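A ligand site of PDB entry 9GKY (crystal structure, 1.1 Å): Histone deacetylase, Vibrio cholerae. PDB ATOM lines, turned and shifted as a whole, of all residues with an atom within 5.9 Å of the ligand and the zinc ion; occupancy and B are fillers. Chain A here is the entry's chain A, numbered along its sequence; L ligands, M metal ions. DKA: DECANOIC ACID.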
ATOM      1  N   TYR A  21     -22.727 -19.707   9.563  1.00  0.00           N
ATOM      2  CA  TYR A  21     -21.969 -19.756  10.809  1.00  0.00           C
ATOM      3  C   TYR A  21     -20.935 -18.630  10.913  1.00  0.00           C
ATOM      4  O   TYR A  21     -20.681 -18.128  11.999  1.00  0.00           O
ATOM      5  CB  TYR A  21     -21.339 -21.134  11.078  1.00  0.00           C
ATOM      6  CG  TYR A  21     -22.389 -22.215  11.333  1.00  0.00           C
ATOM      7  CD1 TYR A  21     -23.726 -21.963  11.560  1.00  0.00           C
ATOM      8  CD2 TYR A  21     -21.981 -23.548  11.364  1.00  0.00           C
ATOM      9  CE1 TYR A  21     -24.648 -22.980  11.846  1.00  0.00           C
ATOM     10  CE2 TYR A  21     -22.900 -24.558  11.637  1.00  0.00           C
ATOM     11  CZ  TYR A  21     -24.218 -24.303  11.872  1.00  0.00           C
ATOM     12  OH  TYR A  21     -25.110 -25.307  12.157  1.00  0.00           O
ATOM     13  N   LEU A  24     -21.814 -13.605  10.135  1.00  0.00           N
ATOM     14  CA  LEU A  24     -22.006 -12.506  11.052  1.00  0.00           C
ATOM     15  C   LEU A  24     -20.830 -11.565  10.997  1.00  0.00           C
ATOM     16  O   LEU A  24     -19.689 -12.007  11.084  1.00  0.00           O
ATOM     17  CB  LEU A  24     -22.156 -13.134  12.436  1.00  0.00           C
ATOM     18  CG  LEU A  24     -22.459 -12.170  13.563  1.00  0.00           C
ATOM     19  CD1 LEU A  24     -23.885 -11.675  13.308  1.00  0.00           C
ATOM     20  CD2 LEU A  24     -22.312 -12.965  14.833  1.00  0.00           C
ATOM     21  N   TYR A  32     -14.690 -12.412  19.589  1.00  0.00           N
ATOM     22  CA  TYR A  32     -15.190 -13.723  19.180  1.00  0.00           C
ATOM     23  C   TYR A  32     -14.642 -14.080  17.789  1.00  0.00           C
ATOM     24  O   TYR A  32     -14.768 -13.291  16.821  1.00  0.00           O
ATOM     25  CB  TYR A  32     -16.720 -13.804  19.153  1.00  0.00           C
ATOM     26  CG  TYR A  32     -16.981 -15.289  19.091  1.00  0.00           C
ATOM     27  CD1 TYR A  32     -16.873 -16.087  20.216  1.00  0.00           C
ATOM     28  CD2 TYR A  32     -17.151 -15.927  17.881  1.00  0.00           C
ATOM     29  CE1 TYR A  32     -16.938 -17.460  20.155  1.00  0.00           C
ATOM     30  CE2 TYR A  32     -17.160 -17.296  17.789  1.00  0.00           C
ATOM     31  CZ  TYR A  32     -17.062 -18.069  18.924  1.00  0.00           C
ATOM     32  OH  TYR A  32     -16.990 -19.402  18.883  1.00  0.00           O
ATOM     33  N   ILE A  34     -15.230 -15.251  14.890  1.00  0.00           N
ATOM     34  CA  ILE A  34     -16.345 -15.618  14.046  1.00  0.00           C
ATOM     35  C   ILE A  34     -15.965 -16.362  12.770  1.00  0.00           C
ATOM     36  O   ILE A  34     -16.793 -17.111  12.249  1.00  0.00           O
ATOM     37  CB  ILE A  34     -17.239 -14.390  13.778  1.00  0.00           C
ATOM     38  CG1 ILE A  34     -18.623 -14.778  13.169  1.00  0.00           C
ATOM     39  CG2 ILE A  34     -16.535 -13.289  13.010  1.00  0.00           C
ATOM     40  CD1 ILE A  34     -19.413 -15.724  14.030  1.00  0.00           C
ATOM     41  N   TYR A  37     -15.362 -20.841  11.715  1.00  0.00           N
ATOM     42  CA  TYR A  37     -16.206 -21.901  11.194  1.00  0.00           C
ATOM     43  C   TYR A  37     -15.972 -22.063   9.703  1.00  0.00           C
ATOM     44  O   TYR A  37     -15.735 -23.199   9.261  1.00  0.00           O
ATOM     45  CB  TYR A  37     -17.673 -21.575  11.507  1.00  0.00           C
ATOM     46  CG  TYR A  37     -17.887 -21.305  12.997  1.00  0.00           C
ATOM     47  CD1 TYR A  37     -17.857 -22.379  13.848  1.00  0.00           C
ATOM     48  CD2 TYR A  37     -18.098 -20.024  13.509  1.00  0.00           C
ATOM     49  CE1 TYR A  37     -17.959 -22.195  15.223  1.00  0.00           C
ATOM     50  CE2 TYR A  37     -18.232 -19.834  14.878  1.00  0.00           C
ATOM     51  CZ  TYR A  37     -18.169 -20.941  15.721  1.00  0.00           C
ATOM     52  OH  TYR A  37     -18.325 -20.762  17.094  1.00  0.00           O
ATOM     53  N   PHE A  98     -22.463  -9.713  21.959  1.00  0.00           N
ATOM     54  CA  PHE A  98     -22.607  -9.352  20.554  1.00  0.00           C
ATOM     55  C   PHE A  98     -23.554  -8.177  20.415  1.00  0.00           C
ATOM     56  O   PHE A  98     -24.460  -8.000  21.248  1.00  0.00           O
ATOM     57  CB  PHE A  98     -23.243 -10.503  19.794  1.00  0.00           C
ATOM     58  CG  PHE A  98     -22.380 -11.743  19.715  1.00  0.00           C
ATOM     59  CD1 PHE A  98     -21.147 -11.734  19.085  1.00  0.00           C
ATOM     60  CD2 PHE A  98     -22.829 -12.934  20.266  1.00  0.00           C
ATOM     61  CE1 PHE A  98     -20.398 -12.882  18.990  1.00  0.00           C
ATOM     62  CE2 PHE A  98     -22.084 -14.097  20.162  1.00  0.00           C
ATOM     63  CZ  PHE A  98     -20.866 -14.068  19.530  1.00  0.00           C
ATOM     64  N   LEU A 104     -27.608 -12.347  13.642  1.00  0.00           N
ATOM     65  CA  LEU A 104     -27.240 -13.083  14.850  1.00  0.00           C
ATOM     66  C   LEU A 104     -28.323 -14.124  15.192  1.00  0.00           C
ATOM     67  O   LEU A 104     -28.003 -15.256  15.590  1.00  0.00           O
ATOM     68  CB  LEU A 104     -27.027 -12.144  16.029  1.00  0.00           C
ATOM     69  CG  LEU A 104     -26.697 -12.819  17.350  1.00  0.00           C
ATOM     70  CD1 LEU A 104     -25.387 -13.545  17.322  1.00  0.00           C
ATOM     71  CD2 LEU A 104     -26.605 -11.710  18.379  1.00  0.00           C
ATOM     72  N   ARG A 107     -28.419 -16.951  12.678  1.00  0.00           N
ATOM     73  CA  ARG A 107     -27.321 -17.862  12.863  1.00  0.00           C
ATOM     74  C   ARG A 107     -27.543 -18.781  14.050  1.00  0.00           C
ATOM     75  O   ARG A 107     -27.315 -19.990  13.964  1.00  0.00           O
ATOM     76  CB  ARG A 107     -26.007 -17.134  13.130  1.00  0.00           C
ATOM     77  CG  ARG A 107     -24.799 -18.027  13.280  1.00  0.00           C
ATOM     78  CD  ARG A 107     -23.690 -17.422  14.194  1.00  0.00           C
ATOM     79  NE  ARG A 107     -22.544 -18.329  14.261  1.00  0.00           N
ATOM     80  CZ  ARG A 107     -22.473 -19.489  14.929  1.00  0.00           C
ATOM     81  NH1 ARG A 107     -23.399 -19.804  15.819  1.00  0.00           N
ATOM     82  NH2 ARG A 107     -21.468 -20.319  14.624  1.00  0.00           N
ATOM     83  N   SER A 132     -19.966 -26.219  14.738  1.00  0.00           N
ATOM     84  CA  SER A 132     -20.308 -25.072  15.589  1.00  0.00           C
ATOM     85  C   SER A 132     -20.817 -25.692  16.899  1.00  0.00           C
ATOM     86  O   SER A 132     -20.474 -26.812  17.234  1.00  0.00           O
ATOM     87  CB  SER A 132     -21.352 -24.093  14.992  1.00  0.00           C
ATOM     88  OG  SER A 132     -21.140 -22.854  15.737  1.00  0.00           O
ATOM     89  N   GLY A 133     -21.621 -24.922  17.635  1.00  0.00           N
ATOM     90  CA  GLY A 133     -22.255 -25.423  18.834  1.00  0.00           C
ATOM     91  C   GLY A 133     -21.389 -25.306  20.101  1.00  0.00           C
ATOM     92  O   GLY A 133     -20.232 -24.885  20.089  1.00  0.00           O
ATOM     93  N   GLY A 134     -21.968 -25.757  21.217  1.00  0.00           N
ATOM     94  CA  GLY A 134     -21.364 -25.661  22.513  1.00  0.00           C
ATOM     95  C   GLY A 134     -21.663 -24.411  23.283  1.00  0.00           C
ATOM     96  O   GLY A 134     -20.768 -23.872  23.974  1.00  0.00           O
ATOM     97  N   TYR A 135     -22.900 -23.918  23.213  1.00  0.00           N
ATOM     98  CA  TYR A 135     -23.271 -22.628  23.760  1.00  0.00           C
ATOM     99  C   TYR A 135     -23.679 -22.801  25.217  1.00  0.00           C
ATOM    100  O   TYR A 135     -24.821 -22.520  25.599  1.00  0.00           O
ATOM    101  CB  TYR A 135     -24.347 -21.984  22.896  1.00  0.00           C
ATOM    102  CG  TYR A 135     -24.045 -22.022  21.410  1.00  0.00           C
ATOM    103  CD1 TYR A 135     -22.748 -21.846  20.931  1.00  0.00           C
ATOM    104  CD2 TYR A 135     -25.037 -22.274  20.473  1.00  0.00           C
ATOM    105  CE1 TYR A 135     -22.445 -21.922  19.573  1.00  0.00           C
ATOM    106  CE2 TYR A 135     -24.751 -22.313  19.106  1.00  0.00           C
ATOM    107  CZ  TYR A 135     -23.450 -22.175  18.665  1.00  0.00           C
ATOM    108  OH  TYR A 135     -23.165 -22.239  17.317  1.00  0.00           O
ATOM    109  N   HIS A 136     -22.700 -23.198  26.046  1.00  0.00           N
ATOM    110  CA  HIS A 136     -22.989 -23.725  27.387  1.00  0.00           C
ATOM    111  C   HIS A 136     -23.233 -22.635  28.409  1.00  0.00           C
ATOM    112  O   HIS A 136     -23.581 -23.017  29.546  1.00  0.00           O
ATOM    113  CB  HIS A 136     -21.852 -24.704  27.786  1.00  0.00           C
ATOM    114  CG  HIS A 136     -20.501 -24.049  27.816  1.00  0.00           C
ATOM    115  ND1 HIS A 136     -19.384 -24.804  28.190  1.00  0.00           N
ATOM    116  CD2 HIS A 136     -20.022 -22.834  27.528  1.00  0.00           C
ATOM    117  CE1 HIS A 136     -18.312 -24.048  28.063  1.00  0.00           C
ATOM    118  NE2 HIS A 136     -18.646 -22.845  27.659  1.00  0.00           N
ATOM    119  N   HIS A 137     -23.079 -21.351  28.090  1.00  0.00           N
ATOM    120  CA  HIS A 137     -23.296 -20.252  29.041  1.00  0.00           C
ATOM    121  C   HIS A 137     -24.690 -19.636  28.935  1.00  0.00           C
ATOM    122  O   HIS A 137     -24.967 -18.654  29.640  1.00  0.00           O
ATOM    123  CB  HIS A 137     -22.232 -19.166  28.883  1.00  0.00           C
ATOM    124  CG  HIS A 137     -20.835 -19.630  29.057  1.00  0.00           C
ATOM    125  ND1 HIS A 137     -20.414 -20.356  30.160  1.00  0.00           N
ATOM    126  CD2 HIS A 137     -19.730 -19.378  28.332  1.00  0.00           C
ATOM    127  CE1 HIS A 137     -19.091 -20.522  30.026  1.00  0.00           C
ATOM    128  NE2 HIS A 137     -18.627 -19.972  28.914  1.00  0.00           N
ATOM    129  N   GLY A 145     -21.585 -14.922  27.877  1.00  0.00           N
ATOM    130  CA  GLY A 145     -20.419 -15.583  27.328  1.00  0.00           C
ATOM    131  C   GLY A 145     -20.604 -16.055  25.872  1.00  0.00           C
ATOM    132  O   GLY A 145     -20.220 -17.168  25.517  1.00  0.00           O
ATOM    133  N   PHE A 146     -21.217 -15.197  25.026  1.00  0.00           N
ATOM    134  CA  PHE A 146     -21.374 -15.428  23.609  1.00  0.00           C
ATOM    135  C   PHE A 146     -22.438 -16.465  23.287  1.00  0.00           C
ATOM    136  O   PHE A 146     -22.602 -16.874  22.146  1.00  0.00           O
ATOM    137  CB  PHE A 146     -20.076 -15.733  22.836  1.00  0.00           C
ATOM    138  CG  PHE A 146     -18.997 -14.740  23.122  1.00  0.00           C
ATOM    139  CD1 PHE A 146     -19.153 -13.413  22.753  1.00  0.00           C
ATOM    140  CD2 PHE A 146     -17.794 -15.118  23.718  1.00  0.00           C
ATOM    141  CE1 PHE A 146     -18.168 -12.475  23.057  1.00  0.00           C
ATOM    142  CE2 PHE A 146     -16.833 -14.179  23.998  1.00  0.00           C
ATOM    143  CZ  PHE A 146     -17.000 -12.881  23.645  1.00  0.00           C
ATOM    144  N   CYS A 147     -23.301 -16.768  24.286  1.00  0.00           N
ATOM    145  CA  CYS A 147     -24.322 -17.783  24.221  1.00  0.00           C
ATOM    146  C   CYS A 147     -25.713 -17.195  24.416  1.00  0.00           C
ATOM    147  O   CYS A 147     -25.968 -16.550  25.392  1.00  0.00           O
ATOM    148  CB  CYS A 147     -24.071 -18.865  25.264  1.00  0.00           C
ATOM    149  SG  CYS A 147     -22.468 -19.660  25.101  1.00  0.00           S
ATOM    150  N   ASP A 174     -14.611 -28.007  27.068  1.00  0.00           N
ATOM    151  CA  ASP A 174     -14.239 -26.621  26.834  1.00  0.00           C
ATOM    152  C   ASP A 174     -13.636 -26.132  28.153  1.00  0.00           C
ATOM    153  O   ASP A 174     -14.028 -26.561  29.260  1.00  0.00           O
ATOM    154  CB  ASP A 174     -15.496 -25.902  26.391  1.00  0.00           C
ATOM    155  CG  ASP A 174     -15.382 -24.399  26.155  1.00  0.00           C
ATOM    156  OD1 ASP A 174     -15.136 -23.618  27.100  1.00  0.00           O
ATOM    157  OD2 ASP A 174     -15.542 -23.955  24.981  1.00  0.00           O
ATOM    158  N   VAL A 175     -12.707 -25.162  28.118  1.00  0.00           N
ATOM    159  CA  VAL A 175     -11.991 -24.718  29.321  1.00  0.00           C
ATOM    160  C   VAL A 175     -12.904 -24.009  30.326  1.00  0.00           C
ATOM    161  O   VAL A 175     -12.550 -23.939  31.520  1.00  0.00           O
ATOM    162  CB  VAL A 175     -10.826 -23.787  28.950  1.00  0.00           C
ATOM    163  CG1 VAL A 175     -11.271 -22.383  28.624  1.00  0.00           C
ATOM    164  CG2 VAL A 175      -9.745 -23.751  30.036  1.00  0.00           C
ATOM    165  N   HIS A 176     -14.060 -23.538  29.885  1.00  0.00           N
ATOM    166  CA  HIS A 176     -15.013 -22.821  30.716  1.00  0.00           C
ATOM    167  C   HIS A 176     -16.048 -23.791  31.303  1.00  0.00           C
ATOM    168  O   HIS A 176     -16.533 -24.659  30.582  1.00  0.00           O
ATOM    169  CB  HIS A 176     -15.716 -21.682  29.956  1.00  0.00           C
ATOM    170  CG  HIS A 176     -14.747 -20.709  29.394  1.00  0.00           C
ATOM    171  ND1 HIS A 176     -14.306 -20.667  28.065  1.00  0.00           N
ATOM    172  CD2 HIS A 176     -14.190 -19.627  30.010  1.00  0.00           C
ATOM    173  CE1 HIS A 176     -13.460 -19.653  27.963  1.00  0.00           C
ATOM    174  NE2 HIS A 176     -13.347 -19.015  29.099  1.00  0.00           N
ATOM    175  N   ASP A 251     -10.257 -24.122  23.724  1.00  0.00           N
ATOM    176  CA  ASP A 251      -9.749 -23.073  24.582  1.00  0.00           C
ATOM    177  C   ASP A 251      -8.972 -23.606  25.785  1.00  0.00           C
ATOM    178  O   ASP A 251      -8.402 -22.808  26.500  1.00  0.00           O
ATOM    179  CB  ASP A 251     -10.833 -22.092  24.939  1.00  0.00           C
ATOM    180  CG  ASP A 251     -12.182 -22.622  25.367  1.00  0.00           C
ATOM    181  OD1 ASP A 251     -12.277 -23.859  25.596  1.00  0.00           O
ATOM    182  OD2 ASP A 251     -13.094 -21.740  25.470  1.00  0.00           O
ATOM    183  N   GLY A 291     -17.334 -26.201  20.137  1.00  0.00           N
ATOM    184  CA  GLY A 291     -17.146 -25.321  21.277  1.00  0.00           C
ATOM    185  C   GLY A 291     -16.204 -24.145  21.042  1.00  0.00           C
ATOM    186  O   GLY A 291     -16.170 -23.615  19.912  1.00  0.00           O
ATOM    187  N   GLY A 292     -15.526 -23.669  22.077  1.00  0.00           N
ATOM    188  CA  GLY A 292     -14.814 -22.412  22.086  1.00  0.00           C
ATOM    189  C   GLY A 292     -13.359 -22.524  21.628  1.00  0.00           C
ATOM    190  O   GLY A 292     -12.926 -23.520  21.086  1.00  0.00           O
ATOM    191  N   GLY A 293     -12.647 -21.432  21.888  1.00  0.00           N
ATOM    192  CA  GLY A 293     -11.319 -21.162  21.336  1.00  0.00           C
ATOM    193  C   GLY A 293     -11.160 -19.673  21.023  1.00  0.00           C
ATOM    194  O   GLY A 293     -12.075 -19.075  20.438  1.00  0.00           O
ATOM    195  N   TYR A 294     -10.049 -19.090  21.435  1.00  0.00           N
ATOM    196  CA  TYR A 294      -9.866 -17.650  21.334  1.00  0.00           C
ATOM    197  C   TYR A 294      -8.459 -17.369  20.852  1.00  0.00           C
ATOM    198  O   TYR A 294      -7.483 -17.509  21.596  1.00  0.00           O
ATOM    199  CB  TYR A 294     -10.143 -16.955  22.712  1.00  0.00           C
ATOM    200  CG  TYR A 294     -11.589 -17.221  23.065  1.00  0.00           C
ATOM    201  CD1 TYR A 294     -12.588 -16.416  22.512  1.00  0.00           C
ATOM    202  CD2 TYR A 294     -11.984 -18.326  23.811  1.00  0.00           C
ATOM    203  CE1 TYR A 294     -13.914 -16.667  22.675  1.00  0.00           C
ATOM    204  CE2 TYR A 294     -13.326 -18.619  23.981  1.00  0.00           C
ATOM    205  CZ  TYR A 294     -14.274 -17.796  23.377  1.00  0.00           C
ATOM    206  OH  TYR A 294     -15.626 -18.045  23.493  1.00  0.00           O
HETATM  207  C1  DKA L   1     -16.874 -20.684  25.318  1.00  0.00           C
HETATM  208  O1  DKA L   1     -15.881 -20.440  24.680  1.00  0.00           O
HETATM  209  C2  DKA L   1     -18.203 -20.004  24.991  1.00  0.00           C
HETATM  210  C3  DKA L   1     -18.572 -19.672  23.555  1.00  0.00           C
HETATM  211  C4  DKA L   1     -18.995 -20.871  22.764  1.00  0.00           C
HETATM  212  C5  DKA L   1     -19.238 -20.577  21.285  1.00  0.00           C
HETATM  213  C6  DKA L   1     -20.014 -19.353  20.948  1.00  0.00           C
HETATM  214  C7  DKA L   1     -20.283 -19.075  19.461  1.00  0.00           C
HETATM  215  C8  DKA L   1     -20.581 -17.628  19.076  1.00  0.00           C
HETATM  216  C9  DKA L   1     -21.038 -17.538  17.641  1.00  0.00           C
HETATM  217  C10 DKA L   1     -21.577 -16.219  17.133  1.00  0.00           C
HETATM  218  O2  DKA L   1     -16.837 -21.358  26.356  1.00  0.00           O
HETATM  219 ZN    ZN M   1     -14.800 -21.861  26.425  1.00  0.00          ZN
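A ring nitrogen (NE2) of His 136 lies close to an oxygen (O2) of the ligand (2.7 Å). A ring nitrogen (NE2) of His 137 lies close to an oxygen (O2) of the ligand (3.4 Å). An oxygen (O1) of the ligand lies close to the side-chain hydroxyl (OH) of Tyr 294, 2.7 Å away.
Within 4 Å of the zinc ion: Asp 174, His 176 and Asp 251. The nearest printed residue that does not touch the zinc ion is His 136 (4.2 Å).
The zinc ion is bound by the side-chain carboxylate of Asp 174 (1.9 Å), the side-chain carboxylate of Asp 251 (2.0 Å), a ring nitrogen (ND1) of His 176 (2.1 Å), an oxygen (O2) of the ligand (2.1 Å) and an oxygen (O1) of the ligand (2.5 Å). Slightly farther from the zinc ion lies the side-chain carboxylate (OD2) of Asp 174 (2.6 Å).
Merely in contact with the ligand: Tyr 32 (3.4 Å), Ile 34 (3.8 Å), Tyr 37 (3.5 Å), Phe 98 (3.3 Å), Arg 107 (3.6 Å), Gly 134 (3.7 Å), Tyr 135 (3.6 Å), Gly 145 (3.5 Å), Phe 146 (3.8 Å) and Gly 292 (3.4 Å). Hydrophobic or aromatic side chains within 4 Å of the ligand: Tyr 32, Ile 34, Phe 98, Tyr 135, His 136, His 137, His 176 and Tyr 294. 16 residues have an atom within 4 Å of the ligand: Tyr 32, Ile 34, Tyr 37, Phe 98, Arg 107, Gly 134, Tyr 135, His 136, His 137, Gly 145, Phe 146, Asp 174, His 176, Asp 251, Gly 292 and Tyr 294. The nearest printed residue that does not touch the ligand is Leu 24 (4.1 Å).
The side-chain hydroxyl of Tyr 135 lies within hydrogen-bond range of the side-chain hydroxyl of Ser 132. A ring nitrogen (NE2) of His 136 sits at hydrogen-bond distance from a ring nitrogen (NE2) of His 137 (3.1 Å). The backbone carbonyl oxygen (O) of Tyr 21 is in hydrogen-bond range of the guanidinium group (NE) of Arg 107, 2.9 Å away. OH of Tyr 135 lies within hydrogen-bond range of NH1 of Arg 107 (2.9 Å). OD1 of Asp 251 lies within hydrogen-bond range of N of Val 175 (2.9 Å). The side-chain sulfur (SG) of Cys 147 is in hydrogen-bond range of the backbone NH (N) of His 137 (3.5 Å). The backbone carbonyl oxygen (O) of Tyr 135 sits close to the side-chain sulfur (SG) of Cys 147 (3.7 Å). OD2 of Asp 174 is in hydrogen-bond range of N of Gly 292.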
